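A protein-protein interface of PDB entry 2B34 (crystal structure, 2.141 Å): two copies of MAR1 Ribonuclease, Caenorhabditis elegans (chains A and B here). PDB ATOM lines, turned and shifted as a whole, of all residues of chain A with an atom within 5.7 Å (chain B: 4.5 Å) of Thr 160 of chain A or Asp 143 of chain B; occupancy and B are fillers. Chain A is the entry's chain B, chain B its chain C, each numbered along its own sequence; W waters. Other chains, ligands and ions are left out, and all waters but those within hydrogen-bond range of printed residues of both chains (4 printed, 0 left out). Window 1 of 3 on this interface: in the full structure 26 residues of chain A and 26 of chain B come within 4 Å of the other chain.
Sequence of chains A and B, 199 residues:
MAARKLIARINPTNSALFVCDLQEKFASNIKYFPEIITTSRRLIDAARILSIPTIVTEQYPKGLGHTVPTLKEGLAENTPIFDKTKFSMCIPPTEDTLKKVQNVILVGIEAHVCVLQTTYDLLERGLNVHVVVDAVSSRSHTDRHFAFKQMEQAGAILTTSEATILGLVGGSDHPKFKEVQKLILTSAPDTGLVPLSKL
The side-chain hydroxyl of Thr 160 of chain A sits at hydrogen-bond distance from the side-chain carboxylate of Asp 143 of chain B (2.6 Å).
The side-chain hydroxyl (OG) of Ser 138 of chain B is in hydrogen-bond range of a ring nitrogen (ND1) of His 112 of chain B (3.0 Å). A ring nitrogen (NE2) of His 112 of chain B sits at hydrogen-bond distance from the side-chain carboxylate of Asp 143 of chain B, 3.3 Å away. The side-chain hydroxyl (OG) of Ser 140 of chain B sits at hydrogen-bond distance from the backbone NH (N) of Asp 143 of chain B (3.4 Å). The backbone NH (N) of Val 133 of chain A lies within hydrogen-bond range of the backbone carbonyl oxygen (O) of Thr 159 of chain A (2.9 Å). OG1 of Thr 164 of chain A lies within hydrogen-bond range of O of Thr 160 of chain A (2.8 Å).
CE2 of Phe 146 of chain B touches CG2 of Val 133 of chain A, 3.7 Å away. O of Leu 158 of chain A touches O of Phe 146 of chain B (3.9 Å). Phe 146 of chain B touches Thr 160 of chain A. Glu 162 of chain A touches His 112 of chain B. Asp 143 of chain B touches Glu 162 of chain A. Ala 163 of chain A touches His 112 of chain B.
Val 131 of chain A touches none of the printed residues of chain B. Of the printed residues of chain B, Val 133 of chain A touches Phe 146 (3.7 Å). Of the printed residues of chain B, Glu 162 of chain A touches His 112 (3.97 Å) and Asp 143 (3.7 Å). Of the printed residues of chain A, Asp 143 of chain B touches Thr 160 and Glu 162. Arg 144 of chain B touches none of the printed residues of chain A. The nearest residue of chain B that does not touch Thr 160 of chain A is Thr 142 of chain B (4.1 Å). The nearest printed residue of chain A that does not touch His 112 of chain B is Thr 160 of chain A (4.6 Å).
Hydrophobic or aromatic side chains of chain B within 4 Å of the printed part of chain A: His 112 and Phe 146. Of the 13 printed residues of chain A, 5 touch a printed residue of chain B. Among the printed residues, no Asp or Glu carboxylate lies within 4 Å of a Lys or Arg side-chain nitrogen of the other chain.
No position is printed for both chains.
Water W3 lies within hydrogen-bond range of OD1 of Asp 143 of chain B, OG of Ser 161 of chain A, OD2 of Asp 134 of chain A and N of Glu 162 of chain A. Water W2 lies within hydrogen-bond range of OE1 of Glu 162 of chain A (2.6 Å), OG of Ser 187 of chain A (2.9 Å) and OD2 of Asp 143 of chain B (3.2 Å). Water W4 lies within hydrogen-bond range of O of His 112 of chain B (2.7 Å) and O of Ala 163 of chain A (2.8 Å). Water W1 lies within hydrogen-bond range of the backbone carbonyl oxygen of Asp 143 of chain B, the side-chain hydroxyl of Thr 160 of chain A and the backbone NH of Ala 147 of chain B.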
ATOM      1  N   VAL A 131       8.553  28.141 -19.050  1.00  0.00           N
ATOM      2  CA  VAL A 131       8.732  27.545 -17.732  1.00  0.00           C
ATOM      3  C   VAL A 131       9.365  26.166 -17.879  1.00  0.00           C
ATOM      4  O   VAL A 131       8.858  25.316 -18.609  1.00  0.00           O
ATOM      5  CB  VAL A 131       7.398  27.480 -16.946  1.00  0.00           C
ATOM      6  CG1 VAL A 131       7.621  26.939 -15.531  1.00  0.00           C
ATOM      7  CG2 VAL A 131       6.743  28.872 -16.893  1.00  0.00           C
ATOM      8  N   VAL A 132      10.496  25.968 -17.207  1.00  0.00           N
ATOM      9  CA  VAL A 132      11.214  24.700 -17.277  1.00  0.00           C
ATOM     10  C   VAL A 132      10.653  23.802 -16.184  1.00  0.00           C
ATOM     11  O   VAL A 132      11.105  23.847 -15.037  1.00  0.00           O
ATOM     12  CB  VAL A 132      12.741  24.882 -17.125  1.00  0.00           C
ATOM     13  CG1 VAL A 132      13.466  23.567 -17.385  1.00  0.00           C
ATOM     14  CG2 VAL A 132      13.248  25.941 -18.088  1.00  0.00           C
ATOM     15  N   VAL A 133       9.658  22.997 -16.552  1.00  0.00           N
ATOM     16  CA  VAL A 133       8.879  22.228 -15.575  1.00  0.00           C
ATOM     17  C   VAL A 133       9.724  21.265 -14.740  1.00  0.00           C
ATOM     18  O   VAL A 133       9.460  21.094 -13.544  1.00  0.00           O
ATOM     19  CB  VAL A 133       7.661  21.493 -16.215  1.00  0.00           C
ATOM     20  CG1 VAL A 133       6.648  22.502 -16.774  1.00  0.00           C
ATOM     21  CG2 VAL A 133       8.106  20.508 -17.294  1.00  0.00           C
ATOM     22  N   ASP A 134      10.743  20.665 -15.359  1.00  0.00           N
ATOM     23  CA  ASP A 134      11.634  19.743 -14.650  1.00  0.00           C
ATOM     24  C   ASP A 134      12.714  20.447 -13.810  1.00  0.00           C
ATOM     25  O   ASP A 134      13.612  19.800 -13.262  1.00  0.00           O
ATOM     26  CB  ASP A 134      12.217  18.652 -15.576  1.00  0.00           C
ATOM     27  CG  ASP A 134      13.004  19.200 -16.770  1.00  0.00           C
ATOM     28  OD1 ASP A 134      12.861  20.383 -17.145  1.00  0.00           O
ATOM     29  OD2 ASP A 134      13.769  18.404 -17.364  1.00  0.00           O
ATOM     30  N   LEU A 158       4.994  25.647 -21.271  1.00  0.00           N
ATOM     31  CA  LEU A 158       5.518  24.630 -20.362  1.00  0.00           C
ATOM     32  C   LEU A 158       6.506  23.737 -21.099  1.00  0.00           C
ATOM     33  O   LEU A 158       6.113  22.875 -21.883  1.00  0.00           O
ATOM     34  CB  LEU A 158       4.390  23.803 -19.743  1.00  0.00           C
ATOM     35  CG  LEU A 158       3.280  24.546 -18.993  1.00  0.00           C
ATOM     36  CD1 LEU A 158       2.214  23.550 -18.532  1.00  0.00           C
ATOM     37  CD2 LEU A 158       3.838  25.342 -17.815  1.00  0.00           C
ATOM     38  N   THR A 159       7.792  23.954 -20.846  1.00  0.00           N
ATOM     39  CA  THR A 159       8.847  23.252 -21.580  1.00  0.00           C
ATOM     40  C   THR A 159       9.720  22.413 -20.636  1.00  0.00           C
ATOM     41  O   THR A 159       9.483  22.386 -19.428  1.00  0.00           O
ATOM     42  CB  THR A 159       9.703  24.252 -22.412  1.00  0.00           C
ATOM     43  OG1 THR A 159      10.538  23.535 -23.331  1.00  0.00           O
ATOM     44  CG2 THR A 159      10.558  25.131 -21.504  1.00  0.00           C
ATOM     45  N   THR A 160      10.712  21.719 -21.186  1.00  0.00           N
ATOM     46  CA  THR A 160      11.646  20.946 -20.361  1.00  0.00           C
ATOM     47  C   THR A 160      13.089  21.369 -20.628  1.00  0.00           C
ATOM     48  O   THR A 160      13.364  22.085 -21.586  1.00  0.00           O
ATOM     49  CB  THR A 160      11.475  19.422 -20.566  1.00  0.00           C
ATOM     50  OG1 THR A 160      11.751  19.089 -21.931  1.00  0.00           O
ATOM     51  CG2 THR A 160      10.049  18.981 -20.220  1.00  0.00           C
ATOM     52  N   SER A 161      13.999  20.935 -19.760  1.00  0.00           N
ATOM     53  CA  SER A 161      15.418  21.295 -19.853  1.00  0.00           C
ATOM     54  C   SER A 161      16.060  20.979 -21.206  1.00  0.00           C
ATOM     55  O   SER A 161      16.698  21.850 -21.794  1.00  0.00           O
ATOM     56  CB  SER A 161      16.220  20.661 -18.712  1.00  0.00           C
ATOM     57  OG  SER A 161      15.938  19.281 -18.561  1.00  0.00           O
ATOM     58  N   GLU A 162      15.893  19.750 -21.702  1.00  0.00           N
ATOM     59  CA  GLU A 162      16.530  19.366 -22.973  1.00  0.00           C
ATOM     60  C   GLU A 162      15.894  20.059 -24.169  1.00  0.00           C
ATOM     61  O   GLU A 162      16.594  20.431 -25.114  1.00  0.00           O
ATOM     62  CB  GLU A 162      16.555  17.842 -23.194  1.00  0.00           C
ATOM     63  CG  GLU A 162      16.943  17.057 -21.962  1.00  0.00           C
ATOM     64  CD  GLU A 162      17.942  15.929 -22.218  1.00  0.00           C
ATOM     65  OE1 GLU A 162      17.865  15.271 -23.293  1.00  0.00           O
ATOM     66  OE2 GLU A 162      18.788  15.704 -21.305  1.00  0.00           O
ATOM     67  N   ALA A 163      14.571  20.224 -24.123  1.00  0.00           N
ATOM     68  CA  ALA A 163      13.840  20.934 -25.171  1.00  0.00           C
ATOM     69  C   ALA A 163      14.344  22.377 -25.301  1.00  0.00           C
ATOM     70  O   ALA A 163      14.547  22.874 -26.407  1.00  0.00           O
ATOM     71  CB  ALA A 163      12.349  20.913 -24.886  1.00  0.00           C
ATOM     72  N   THR A 164      14.551  23.028 -24.158  1.00  0.00           N
ATOM     73  CA  THR A 164      15.018  24.412 -24.105  1.00  0.00           C
ATOM     74  C   THR A 164      16.462  24.543 -24.586  1.00  0.00           C
ATOM     75  O   THR A 164      16.762  25.376 -25.434  1.00  0.00           O
ATOM     76  CB  THR A 164      14.873  24.985 -22.677  1.00  0.00           C
ATOM     77  OG1 THR A 164      13.518  24.820 -22.246  1.00  0.00           O
ATOM     78  CG2 THR A 164      15.241  26.471 -22.634  1.00  0.00           C
ATOM     79  N   ILE A 165      17.342  23.700 -24.054  1.00  0.00           N
ATOM     80  CA  ILE A 165      18.767  23.763 -24.373  1.00  0.00           C
ATOM     81  C   ILE A 165      19.020  23.500 -25.861  1.00  0.00           C
ATOM     82  O   ILE A 165      19.764  24.241 -26.502  1.00  0.00           O
ATOM     83  CB  ILE A 165      19.599  22.825 -23.453  1.00  0.00           C
ATOM     84  CG1 ILE A 165      19.575  23.349 -22.009  1.00  0.00           C
ATOM     85  CG2 ILE A 165      21.041  22.707 -23.947  1.00  0.00           C
ATOM     86  CD1 ILE A 165      20.042  22.342 -20.963  1.00  0.00           C
ATOM     87  N   SER A 187      19.735  12.002 -19.615  1.00  0.00           N
ATOM     88  CA  SER A 187      18.408  12.582 -19.439  1.00  0.00           C
ATOM     89  C   SER A 187      18.338  13.301 -18.101  1.00  0.00           C
ATOM     90  O   SER A 187      18.998  12.895 -17.140  1.00  0.00           O
ATOM     91  CB  SER A 187      17.337  11.493 -19.494  1.00  0.00           C
ATOM     92  OG  SER A 187      17.235  10.956 -20.796  1.00  0.00           O
ATOM     93  N   HIS B 112      10.337  16.502 -28.638  1.00  0.00           N
ATOM     94  CA  HIS B 112      10.594  17.799 -28.022  1.00  0.00           C
ATOM     95  C   HIS B 112      11.738  18.554 -28.720  1.00  0.00           C
ATOM     96  O   HIS B 112      12.123  19.643 -28.288  1.00  0.00           O
ATOM     97  CB  HIS B 112      10.947  17.581 -26.554  1.00  0.00           C
ATOM     98  CG  HIS B 112      12.216  16.810 -26.355  1.00  0.00           C
ATOM     99  ND1 HIS B 112      12.374  15.511 -26.791  1.00  0.00           N
ATOM    100  CD2 HIS B 112      13.390  17.156 -25.775  1.00  0.00           C
ATOM    101  CE1 HIS B 112      13.591  15.095 -26.497  1.00  0.00           C
ATOM    102  NE2 HIS B 112      14.228  16.073 -25.878  1.00  0.00           N
ATOM    103  N   SER B 138      10.232  10.186 -27.479  1.00  0.00           N
ATOM    104  CA  SER B 138      11.490  10.779 -27.015  1.00  0.00           C
ATOM    105  C   SER B 138      12.244   9.757 -26.179  1.00  0.00           C
ATOM    106  O   SER B 138      11.687   8.726 -25.802  1.00  0.00           O
ATOM    107  CB  SER B 138      11.223  12.003 -26.130  1.00  0.00           C
ATOM    108  OG  SER B 138      10.683  13.093 -26.854  1.00  0.00           O
ATOM    109  N   SER B 140      13.252  10.494 -23.139  1.00  0.00           N
ATOM    110  CA  SER B 140      12.598  10.692 -21.851  1.00  0.00           C
ATOM    111  C   SER B 140      11.088  10.841 -22.004  1.00  0.00           C
ATOM    112  O   SER B 140      10.608  11.603 -22.844  1.00  0.00           O
ATOM    113  CB  SER B 140      13.179  11.919 -21.152  1.00  0.00           C
ATOM    114  OG  SER B 140      12.333  12.380 -20.116  1.00  0.00           O
ATOM    115  N   HIS B 141      10.356  10.092 -21.182  1.00  0.00           N
ATOM    116  CA  HIS B 141       8.903  10.184 -21.079  1.00  0.00           C
ATOM    117  C   HIS B 141       8.438  11.620 -20.807  1.00  0.00           C
ATOM    118  O   HIS B 141       7.452  12.088 -21.392  1.00  0.00           O
ATOM    119  CB  HIS B 141       8.407   9.268 -19.954  1.00  0.00           C
ATOM    120  CG  HIS B 141       8.391   7.812 -20.309  1.00  0.00           C
ATOM    121  ND1 HIS B 141       8.968   6.847 -19.511  1.00  0.00           N
ATOM    122  CD2 HIS B 141       7.854   7.154 -21.364  1.00  0.00           C
ATOM    123  CE1 HIS B 141       8.777   5.657 -20.055  1.00  0.00           C
ATOM    124  NE2 HIS B 141       8.109   5.816 -21.183  1.00  0.00           N
ATOM    125  N   THR B 142       9.164  12.303 -19.921  1.00  0.00           N
ATOM    126  CA  THR B 142       8.863  13.678 -19.533  1.00  0.00           C
ATOM    127  C   THR B 142       8.981  14.639 -20.711  1.00  0.00           C
ATOM    128  O   THR B 142       8.109  15.485 -20.904  1.00  0.00           O
ATOM    129  CB  THR B 142       9.757  14.144 -18.356  1.00  0.00           C
ATOM    130  OG1 THR B 142       9.513  13.305 -17.220  1.00  0.00           O
ATOM    131  CG2 THR B 142       9.461  15.588 -17.974  1.00  0.00           C
ATOM    132  N   ASP B 143      10.049  14.491 -21.499  1.00  0.00           N
ATOM    133  CA  ASP B 143      10.267  15.328 -22.681  1.00  0.00           C
ATOM    134  C   ASP B 143       9.149  15.155 -23.707  1.00  0.00           C
ATOM    135  O   ASP B 143       8.674  16.125 -24.289  1.00  0.00           O
ATOM    136  CB  ASP B 143      11.622  15.015 -23.322  1.00  0.00           C
ATOM    137  CG  ASP B 143      12.794  15.615 -22.561  1.00  0.00           C
ATOM    138  OD1 ASP B 143      12.608  16.604 -21.815  1.00  0.00           O
ATOM    139  OD2 ASP B 143      13.919  15.098 -22.719  1.00  0.00           O
ATOM    140  N   ARG B 144       8.738  13.907 -23.916  1.00  0.00           N
ATOM    141  CA  ARG B 144       7.670  13.567 -24.856  1.00  0.00           C
ATOM    142  C   ARG B 144       6.324  14.149 -24.406  1.00  0.00           C
ATOM    143  O   ARG B 144       5.591  14.737 -25.209  1.00  0.00           O
ATOM    144  CB  ARG B 144       7.571  12.043 -24.990  1.00  0.00           C
ATOM    145  CG  ARG B 144       6.517  11.550 -25.969  1.00  0.00           C
ATOM    146  CD  ARG B 144       6.226  10.073 -25.738  1.00  0.00           C
ATOM    147  NE  ARG B 144       5.311   9.530 -26.741  1.00  0.00           N
ATOM    148  CZ  ARG B 144       4.649   8.386 -26.611  1.00  0.00           C
ATOM    149  NH1 ARG B 144       4.781   7.660 -25.503  1.00  0.00           N
ATOM    150  NH2 ARG B 144       3.842   7.969 -27.584  1.00  0.00           N
ATOM    151  N   HIS B 145       6.018  13.969 -23.121  1.00  0.00           N
ATOM    152  CA  HIS B 145       4.770  14.429 -22.510  1.00  0.00           C
ATOM    153  C   HIS B 145       4.585  15.941 -22.694  1.00  0.00           C
ATOM    154  O   HIS B 145       3.550  16.398 -23.178  1.00  0.00           O
ATOM    155  CB  HIS B 145       4.761  14.058 -21.018  1.00  0.00           C
ATOM    156  CG  HIS B 145       3.442  14.285 -20.343  1.00  0.00           C
ATOM    157  ND1 HIS B 145       3.182  15.396 -19.571  1.00  0.00           N
ATOM    158  CD2 HIS B 145       2.310  13.543 -20.329  1.00  0.00           C
ATOM    159  CE1 HIS B 145       1.946  15.330 -19.110  1.00  0.00           C
ATOM    160  NE2 HIS B 145       1.395  14.214 -19.554  1.00  0.00           N
ATOM    161  N   PHE B 146       5.606  16.709 -22.329  1.00  0.00           N
ATOM    162  CA  PHE B 146       5.548  18.162 -22.468  1.00  0.00           C
ATOM    163  C   PHE B 146       5.766  18.677 -23.897  1.00  0.00           C
ATOM    164  O   PHE B 146       5.375  19.801 -24.210  1.00  0.00           O
ATOM    165  CB  PHE B 146       6.462  18.839 -21.437  1.00  0.00           C
ATOM    166  CG  PHE B 146       5.887  18.823 -20.050  1.00  0.00           C
ATOM    167  CD1 PHE B 146       4.980  19.801 -19.649  1.00  0.00           C
ATOM    168  CD2 PHE B 146       6.199  17.793 -19.163  1.00  0.00           C
ATOM    169  CE1 PHE B 146       4.414  19.772 -18.373  1.00  0.00           C
ATOM    170  CE2 PHE B 146       5.634  17.756 -17.887  1.00  0.00           C
ATOM    171  CZ  PHE B 146       4.746  18.749 -17.495  1.00  0.00           C
ATOM    172  N   ALA B 147       6.363  17.854 -24.761  1.00  0.00           N
ATOM    173  CA  ALA B 147       6.404  18.154 -26.200  1.00  0.00           C
ATOM    174  C   ALA B 147       4.995  18.301 -26.759  1.00  0.00           C
ATOM    175  O   ALA B 147       4.701  19.268 -27.456  1.00  0.00           O
ATOM    176  CB  ALA B 147       7.165  17.082 -26.969  1.00  0.00           C
HETATM  177  O   HOH W   1       9.319  18.930 -23.795  1.00  0.00           O
HETATM  178  O   HOH W   2      16.444  13.202 -22.532  1.00  0.00           O
HETATM  179  O   HOH W   3      14.458  17.368 -20.164  1.00  0.00           O
HETATM  180  O   HOH W   4      13.319  21.991 -28.757  1.00  0.00           O
